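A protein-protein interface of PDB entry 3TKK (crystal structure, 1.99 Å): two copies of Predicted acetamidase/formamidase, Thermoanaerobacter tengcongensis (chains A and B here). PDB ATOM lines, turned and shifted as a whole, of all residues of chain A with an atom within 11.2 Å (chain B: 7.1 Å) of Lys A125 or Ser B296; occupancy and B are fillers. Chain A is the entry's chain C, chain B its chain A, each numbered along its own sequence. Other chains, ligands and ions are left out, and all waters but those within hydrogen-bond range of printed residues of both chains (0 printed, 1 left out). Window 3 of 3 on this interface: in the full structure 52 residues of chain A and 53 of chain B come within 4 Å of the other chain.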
ATOM      1  N   LYS A 111     -33.226 -14.005  39.865  1.00  0.00           N
ATOM      2  CA  LYS A 111     -33.840 -14.694  38.736  1.00  0.00           C
ATOM      3  C   LYS A 111     -33.163 -16.049  38.664  1.00  0.00           C
ATOM      4  O   LYS A 111     -31.943 -16.118  38.790  1.00  0.00           O
ATOM      5  CB  LYS A 111     -33.619 -13.924  37.441  1.00  0.00           C
ATOM      6  CG  LYS A 111     -34.335 -14.543  36.291  1.00  0.00           C
ATOM      7  CD  LYS A 111     -33.884 -13.987  34.935  1.00  0.00           C
ATOM      8  CE  LYS A 111     -34.764 -14.572  33.809  1.00  0.00           C
ATOM      9  NZ  LYS A 111     -34.560 -13.727  32.593  1.00  0.00           N
ATOM     10  N   VAL A 113     -32.111 -19.004  36.286  1.00  0.00           N
ATOM     11  CA  VAL A 113     -31.978 -19.258  34.850  1.00  0.00           C
ATOM     12  C   VAL A 113     -31.620 -20.688  34.527  1.00  0.00           C
ATOM     13  O   VAL A 113     -30.968 -21.353  35.285  1.00  0.00           O
ATOM     14  CB  VAL A 113     -30.946 -18.366  34.193  1.00  0.00           C
ATOM     15  CG1 VAL A 113     -31.413 -16.943  34.323  1.00  0.00           C
ATOM     16  CG2 VAL A 113     -29.571 -18.597  34.813  1.00  0.00           C
ATOM     17  N   LYS A 119     -24.897 -23.835  28.117  1.00  0.00           N
ATOM     18  CA  LYS A 119     -25.132 -22.399  27.967  1.00  0.00           C
ATOM     19  C   LYS A 119     -26.103 -21.840  29.002  1.00  0.00           C
ATOM     20  O   LYS A 119     -27.137 -22.429  29.293  1.00  0.00           O
ATOM     21  CB  LYS A 119     -25.668 -22.087  26.558  1.00  0.00           C
ATOM     22  CG  LYS A 119     -24.579 -21.788  25.522  1.00  0.00           C
ATOM     23  CD  LYS A 119     -24.843 -22.434  24.166  1.00  0.00           C
ATOM     24  CE  LYS A 119     -23.659 -22.220  23.225  1.00  0.00           C
ATOM     25  NZ  LYS A 119     -23.909 -21.035  22.361  1.00  0.00           N
ATOM     26  N   VAL A 120     -25.769 -20.687  29.565  1.00  0.00           N
ATOM     27  CA  VAL A 120     -26.666 -20.045  30.487  1.00  0.00           C
ATOM     28  C   VAL A 120     -27.677 -19.240  29.676  1.00  0.00           C
ATOM     29  O   VAL A 120     -27.280 -18.294  28.969  1.00  0.00           O
ATOM     30  CB  VAL A 120     -25.876 -19.133  31.461  1.00  0.00           C
ATOM     31  CG1 VAL A 120     -26.860 -18.577  32.491  1.00  0.00           C
ATOM     32  CG2 VAL A 120     -24.733 -19.977  32.203  1.00  0.00           C
ATOM     33  N   ILE A 121     -28.955 -19.617  29.709  1.00  0.00           N
ATOM     34  CA  ILE A 121     -29.998 -18.891  28.957  1.00  0.00           C
ATOM     35  C   ILE A 121     -30.399 -17.643  29.713  1.00  0.00           C
ATOM     36  O   ILE A 121     -31.347 -17.647  30.500  1.00  0.00           O
ATOM     37  CB  ILE A 121     -31.225 -19.739  28.728  1.00  0.00           C
ATOM     38  CG1 ILE A 121     -30.831 -20.877  27.816  1.00  0.00           C
ATOM     39  CG2 ILE A 121     -32.347 -18.877  28.075  1.00  0.00           C
ATOM     40  CD1 ILE A 121     -30.609 -22.057  28.559  1.00  0.00           C
ATOM     41  N   PHE A 122     -29.632 -16.585  29.502  1.00  0.00           N
ATOM     42  CA  PHE A 122     -29.790 -15.347  30.266  1.00  0.00           C
ATOM     43  C   PHE A 122     -31.121 -14.674  29.996  1.00  0.00           C
ATOM     44  O   PHE A 122     -31.817 -14.222  30.923  1.00  0.00           O
ATOM     45  CB  PHE A 122     -28.698 -14.375  29.867  1.00  0.00           C
ATOM     46  CG  PHE A 122     -28.809 -13.077  30.523  1.00  0.00           C
ATOM     47  CD1 PHE A 122     -28.380 -12.951  31.837  1.00  0.00           C
ATOM     48  CD2 PHE A 122     -29.365 -11.983  29.857  1.00  0.00           C
ATOM     49  CE1 PHE A 122     -28.449 -11.717  32.461  1.00  0.00           C
ATOM     50  CE2 PHE A 122     -29.454 -10.741  30.494  1.00  0.00           C
ATOM     51  CZ  PHE A 122     -28.976 -10.629  31.817  1.00  0.00           C
ATOM     52  N   ASN A 123     -31.413 -14.585  28.710  1.00  0.00           N
ATOM     53  CA  ASN A 123     -32.709 -14.270  28.200  1.00  0.00           C
ATOM     54  C   ASN A 123     -32.921 -14.940  26.835  1.00  0.00           C
ATOM     55  O   ASN A 123     -32.099 -15.743  26.376  1.00  0.00           O
ATOM     56  CB  ASN A 123     -32.837 -12.768  28.085  1.00  0.00           C
ATOM     57  CG  ASN A 123     -31.860 -12.213  27.112  1.00  0.00           C
ATOM     58  OD1 ASN A 123     -31.533 -11.040  27.173  1.00  0.00           O
ATOM     59  ND2 ASN A 123     -31.370 -13.069  26.191  1.00  0.00           N
ATOM     60  N   GLU A 124     -34.030 -14.607  26.177  1.00  0.00           N
ATOM     61  CA  GLU A 124     -34.327 -15.198  24.896  1.00  0.00           C
ATOM     62  C   GLU A 124     -33.258 -14.862  23.823  1.00  0.00           C
ATOM     63  O   GLU A 124     -33.182 -15.547  22.807  1.00  0.00           O
ATOM     64  CB  GLU A 124     -35.737 -14.772  24.422  1.00  0.00           C
ATOM     65  CG  GLU A 124     -35.796 -13.380  23.718  1.00  0.00           C
ATOM     66  CD  GLU A 124     -35.260 -12.182  24.561  1.00  0.00           C
ATOM     67  OE1 GLU A 124     -35.396 -12.186  25.805  1.00  0.00           O
ATOM     68  OE2 GLU A 124     -34.701 -11.214  23.974  1.00  0.00           O
ATOM     69  N   LYS A 125     -32.417 -13.832  24.036  1.00  0.00           N
ATOM     70  CA  LYS A 125     -31.420 -13.460  23.006  1.00  0.00           C
ATOM     71  C   LYS A 125     -29.993 -13.909  23.303  1.00  0.00           C
ATOM     72  O   LYS A 125     -29.202 -14.037  22.358  1.00  0.00           O
ATOM     73  CB  LYS A 125     -31.452 -11.946  22.597  1.00  0.00           C
ATOM     74  CG  LYS A 125     -32.220 -11.663  21.240  1.00  0.00           C
ATOM     75  CD  LYS A 125     -31.716 -10.428  20.410  1.00  0.00           C
ATOM     76  CE  LYS A 125     -32.041  -9.062  21.080  1.00  0.00           C
ATOM     77  NZ  LYS A 125     -32.238  -9.223  22.602  1.00  0.00           N
ATOM     78  N   LEU A 126     -29.637 -14.118  24.584  1.00  0.00           N
ATOM     79  CA  LEU A 126     -28.293 -14.570  24.891  1.00  0.00           C
ATOM     80  C   LEU A 126     -28.268 -15.963  25.534  1.00  0.00           C
ATOM     81  O   LEU A 126     -28.844 -16.173  26.595  1.00  0.00           O
ATOM     82  CB  LEU A 126     -27.591 -13.606  25.846  1.00  0.00           C
ATOM     83  CG  LEU A 126     -27.743 -12.142  25.583  1.00  0.00           C
ATOM     84  CD1 LEU A 126     -27.373 -11.387  26.815  1.00  0.00           C
ATOM     85  CD2 LEU A 126     -26.920 -11.727  24.348  1.00  0.00           C
ATOM     86  N   ALA A 127     -27.608 -16.905  24.866  1.00  0.00           N
ATOM     87  CA  ALA A 127     -27.223 -18.162  25.458  1.00  0.00           C
ATOM     88  C   ALA A 127     -25.696 -18.098  25.729  1.00  0.00           C
ATOM     89  O   ALA A 127     -24.882 -17.947  24.818  1.00  0.00           O
ATOM     90  CB  ALA A 127     -27.633 -19.327  24.523  1.00  0.00           C
ATOM     91  N   LEU A 128     -25.288 -18.085  26.985  1.00  0.00           N
ATOM     92  CA  LEU A 128     -23.885 -17.746  27.276  1.00  0.00           C
ATOM     93  C   LEU A 128     -23.112 -18.999  27.720  1.00  0.00           C
ATOM     94  O   LEU A 128     -23.528 -19.661  28.662  1.00  0.00           O
ATOM     95  CB  LEU A 128     -23.813 -16.673  28.345  1.00  0.00           C
ATOM     96  CG  LEU A 128     -24.603 -15.375  28.244  1.00  0.00           C
ATOM     97  CD1 LEU A 128     -24.599 -14.608  29.572  1.00  0.00           C
ATOM     98  CD2 LEU A 128     -24.008 -14.478  27.173  1.00  0.00           C
ATOM     99  N   PRO A 129     -22.065 -19.393  26.964  1.00  0.00           N
ATOM    100  CA  PRO A 129     -21.349 -20.643  27.282  1.00  0.00           C
ATOM    101  C   PRO A 129     -20.833 -20.632  28.758  1.00  0.00           C
ATOM    102  O   PRO A 129     -20.433 -19.625  29.300  1.00  0.00           O
ATOM    103  CB  PRO A 129     -20.221 -20.703  26.229  1.00  0.00           C
ATOM    104  CG  PRO A 129     -20.760 -19.797  25.011  1.00  0.00           C
ATOM    105  CD  PRO A 129     -21.710 -18.816  25.639  1.00  0.00           C
ATOM    106  N   ASP B 257     -33.782  -1.729  26.191  1.00  0.00           N
ATOM    107  CA  ASP B 257     -34.867  -1.720  27.141  1.00  0.00           C
ATOM    108  C   ASP B 257     -34.552  -2.702  28.270  1.00  0.00           C
ATOM    109  O   ASP B 257     -35.440  -3.161  29.016  1.00  0.00           O
ATOM    110  CB  ASP B 257     -36.177  -2.066  26.429  1.00  0.00           C
ATOM    111  CG  ASP B 257     -36.219  -3.517  25.922  1.00  0.00           C
ATOM    112  OD1 ASP B 257     -35.216  -4.273  26.120  1.00  0.00           O
ATOM    113  OD2 ASP B 257     -37.244  -3.898  25.307  1.00  0.00           O
ATOM    114  N   ASN B 291     -18.070  -8.078  21.975  1.00  0.00           N
ATOM    115  CA  ASN B 291     -18.863  -7.372  20.955  1.00  0.00           C
ATOM    116  C   ASN B 291     -20.191  -8.029  20.597  1.00  0.00           C
ATOM    117  O   ASN B 291     -21.153  -7.346  20.271  1.00  0.00           O
ATOM    118  CB  ASN B 291     -18.052  -7.166  19.685  1.00  0.00           C
ATOM    119  CG  ASN B 291     -16.872  -6.274  19.910  1.00  0.00           C
ATOM    120  OD1 ASN B 291     -16.844  -5.416  20.855  1.00  0.00           O
ATOM    121  ND2 ASN B 291     -15.936  -6.349  19.021  1.00  0.00           N
ATOM    122  N   TRP B 292     -20.300  -9.352  20.635  1.00  0.00           N
ATOM    123  CA  TRP B 292     -21.566  -9.904  20.083  1.00  0.00           C
ATOM    124  C   TRP B 292     -22.756  -9.634  21.052  1.00  0.00           C
ATOM    125  O   TRP B 292     -23.935  -9.603  20.672  1.00  0.00           O
ATOM    126  CB  TRP B 292     -21.424 -11.395  19.771  1.00  0.00           C
ATOM    127  CG  TRP B 292     -21.225 -12.230  20.984  1.00  0.00           C
ATOM    128  CD1 TRP B 292     -20.065 -12.445  21.655  1.00  0.00           C
ATOM    129  CD2 TRP B 292     -22.242 -12.985  21.678  1.00  0.00           C
ATOM    130  NE1 TRP B 292     -20.308 -13.231  22.765  1.00  0.00           N
ATOM    131  CE2 TRP B 292     -21.630 -13.612  22.760  1.00  0.00           C
ATOM    132  CE3 TRP B 292     -23.619 -13.185  21.471  1.00  0.00           C
ATOM    133  CZ2 TRP B 292     -22.327 -14.435  23.629  1.00  0.00           C
ATOM    134  CZ3 TRP B 292     -24.311 -14.008  22.331  1.00  0.00           C
ATOM    135  CH2 TRP B 292     -23.666 -14.599  23.421  1.00  0.00           C
ATOM    136  N   ILE B 293     -22.461  -9.467  22.325  1.00  0.00           N
ATOM    137  CA  ILE B 293     -23.495  -9.009  23.262  1.00  0.00           C
ATOM    138  C   ILE B 293     -23.999  -7.609  22.907  1.00  0.00           C
ATOM    139  O   ILE B 293     -25.199  -7.396  22.720  1.00  0.00           O
ATOM    140  CB  ILE B 293     -22.958  -8.951  24.714  1.00  0.00           C
ATOM    141  CG1 ILE B 293     -22.259 -10.247  25.125  1.00  0.00           C
ATOM    142  CG2 ILE B 293     -24.070  -8.677  25.672  1.00  0.00           C
ATOM    143  CD1 ILE B 293     -23.035 -11.057  26.022  1.00  0.00           C
ATOM    144  N   LEU B 294     -23.117  -6.628  22.751  1.00  0.00           N
ATOM    145  CA  LEU B 294     -23.618  -5.332  22.350  1.00  0.00           C
ATOM    146  C   LEU B 294     -24.378  -5.474  21.020  1.00  0.00           C
ATOM    147  O   LEU B 294     -25.447  -4.869  20.767  1.00  0.00           O
ATOM    148  CB  LEU B 294     -22.472  -4.348  22.087  1.00  0.00           C
ATOM    149  CG  LEU B 294     -21.452  -3.867  23.092  1.00  0.00           C
ATOM    150  CD1 LEU B 294     -21.723  -2.429  23.387  1.00  0.00           C
ATOM    151  CD2 LEU B 294     -21.368  -4.688  24.360  1.00  0.00           C
ATOM    152  N   GLU B 295     -23.793  -6.257  20.139  1.00  0.00           N
ATOM    153  CA  GLU B 295     -24.379  -6.469  18.801  1.00  0.00           C
ATOM    154  C   GLU B 295     -25.806  -6.998  18.938  1.00  0.00           C
ATOM    155  O   GLU B 295     -26.716  -6.513  18.289  1.00  0.00           O
ATOM    156  CB  GLU B 295     -23.491  -7.444  18.037  1.00  0.00           C
ATOM    157  CG  GLU B 295     -23.901  -7.790  16.608  1.00  0.00           C
ATOM    158  CD  GLU B 295     -24.271  -6.563  15.798  1.00  0.00           C
ATOM    159  OE1 GLU B 295     -23.855  -5.428  16.135  1.00  0.00           O
ATOM    160  OE2 GLU B 295     -24.991  -6.736  14.811  1.00  0.00           O
ATOM    161  N   SER B 296     -26.027  -7.983  19.797  1.00  0.00           N
ATOM    162  CA  SER B 296     -27.389  -8.487  19.903  1.00  0.00           C
ATOM    163  C   SER B 296     -28.354  -7.372  20.217  1.00  0.00           C
ATOM    164  O   SER B 296     -29.466  -7.377  19.689  1.00  0.00           O
ATOM    165  CB  SER B 296     -27.502  -9.538  20.962  1.00  0.00           C
ATOM    166  OG  SER B 296     -26.790 -10.683  20.553  1.00  0.00           O
ATOM    167  N   TYR B 297     -27.956  -6.412  21.066  1.00  0.00           N
ATOM    168  CA  TYR B 297     -28.913  -5.369  21.459  1.00  0.00           C
ATOM    169  C   TYR B 297     -28.783  -4.202  20.579  1.00  0.00           C
ATOM    170  O   TYR B 297     -29.157  -3.083  20.969  1.00  0.00           O
ATOM    171  CB  TYR B 297     -28.792  -4.923  22.902  1.00  0.00           C
ATOM    172  CG  TYR B 297     -29.027  -5.978  23.949  1.00  0.00           C
ATOM    173  CD1 TYR B 297     -27.992  -6.788  24.309  1.00  0.00           C
ATOM    174  CD2 TYR B 297     -30.253  -6.137  24.612  1.00  0.00           C
ATOM    175  CE1 TYR B 297     -28.083  -7.706  25.275  1.00  0.00           C
ATOM    176  CE2 TYR B 297     -30.382  -7.140  25.633  1.00  0.00           C
ATOM    177  CZ  TYR B 297     -29.260  -7.918  25.930  1.00  0.00           C
ATOM    178  OH  TYR B 297     -29.145  -8.912  26.911  1.00  0.00           O
ATOM    179  N   GLY B 298     -28.245  -4.440  19.382  1.00  0.00           N
ATOM    180  CA  GLY B 298     -28.238  -3.422  18.353  1.00  0.00           C
ATOM    181  C   GLY B 298     -27.446  -2.192  18.763  1.00  0.00           C
ATOM    182  O   GLY B 298     -27.704  -1.087  18.255  1.00  0.00           O
ATOM    183  N   ILE B 299     -26.481  -2.383  19.683  1.00  0.00           N
ATOM    184  CA  ILE B 299     -25.600  -1.290  20.113  1.00  0.00           C
ATOM    185  C   ILE B 299     -24.401  -1.113  19.176  1.00  0.00           C
ATOM    186  O   ILE B 299     -23.448  -1.903  19.214  1.00  0.00           O
ATOM    187  CB  ILE B 299     -25.126  -1.477  21.595  1.00  0.00           C
ATOM    188  CG1 ILE B 299     -26.328  -1.616  22.525  1.00  0.00           C
ATOM    189  CG2 ILE B 299     -24.341  -0.280  22.043  1.00  0.00           C
ATOM    190  CD1 ILE B 299     -25.959  -1.551  23.978  1.00  0.00           C
ATOM    191  N   ARG B 300     -24.440  -0.086  18.319  1.00  0.00           N
ATOM    192  CA  ARG B 300     -23.289   0.209  17.452  1.00  0.00           C
ATOM    193  C   ARG B 300     -23.041   1.699  17.327  1.00  0.00           C
ATOM    194  O   ARG B 300     -23.891   2.455  16.857  1.00  0.00           O
ATOM    195  CB  ARG B 300     -23.456  -0.440  16.085  1.00  0.00           C
ATOM    196  CG  ARG B 300     -24.871  -0.414  15.641  1.00  0.00           C
ATOM    197  CD  ARG B 300     -25.116  -1.184  14.358  1.00  0.00           C
ATOM    198  NE  ARG B 300     -26.500  -1.627  14.414  1.00  0.00           N
ATOM    199  CZ  ARG B 300     -26.872  -2.881  14.634  1.00  0.00           C
ATOM    200  NH1 ARG B 300     -25.966  -3.840  14.753  1.00  0.00           N
ATOM    201  NH2 ARG B 300     -28.152  -3.178  14.717  1.00  0.00           N
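OD1 of Asn A123 sits at hydrogen-bond distance from OH of Tyr B297 (3.2 Å).
O of Trp B292 is in hydrogen-bond range of OG of Ser B296. N of Val A120 lies within hydrogen-bond range of O of Leu A128, 2.6 Å away. The side-chain amide nitrogen (ND2) of Asn A123 sits close to the backbone NH (N) of Lys A125. ND2 of Asn A123 lies close to N of Leu A126 (2.6 Å). The side-chain amino group (NZ) of Lys A125 is in salt-bridge range of the side-chain carboxylate (OE2) of Glu A124 (3.5 Å).
Among the printed residues, merely in contact across the chains: Lys A125 with Ser B296 (3.4 Å), Leu A126 with Ser B296 (3.9 Å), Leu A126 with Tyr B297 (3.0 Å), Ala A127 with Trp B292 (3.8 Å), Leu A128 with Trp B292 (3.8 Å) and Leu A128 with Ile B293 (3.7 Å).
Of chain A, only Lys A125 and Leu A126 come within 4 Å of Ser B296. Ile B293 touches just one residue of chain A: Leu A128 (3.7 Å). Of chain A, only Asn A123 (3.2 Å) and Leu A126 (3.0 Å) come within 4 Å of Tyr B297. No residue of chain A comes within 4 Å of Gly B298. Of the printed residues of chain B, Leu A126 touches Ser B296 (3.9 Å) and Tyr B297 (3.0 Å). Of the printed residues of chain B, Asn A123 touches Tyr B297. Of the printed residues of chain B, Leu A128 touches Trp B292 and Ile B293. Printed residues of chain B within 4 Å of Ala A127: Trp B292 (3.8 Å). Ile B299 touches none of the printed residues of chain A. Val A120 touches none of the printed residues of chain B. The nearest printed residue of chain A that does not touch Trp B292 is Leu A126 (4.01 Å).
Of the 11 printed residues of chain B, 4 touch a printed residue of chain A. Of the 13 printed residues of chain A, 5 touch a printed residue of chain B. Printed residues of chain A that touch a printed residue of chain B: Asn A123, Lys A125, Leu A126, Ala A127 and Leu A128. Hydrophobic or aromatic side chains of chain A that line the printed part of chain B: Leu A126 and Leu A128.
No position is printed for both chains. Of the 7 pairs that touch across the chains among the printed residues, none has its exchanged pair printed and touching as well.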
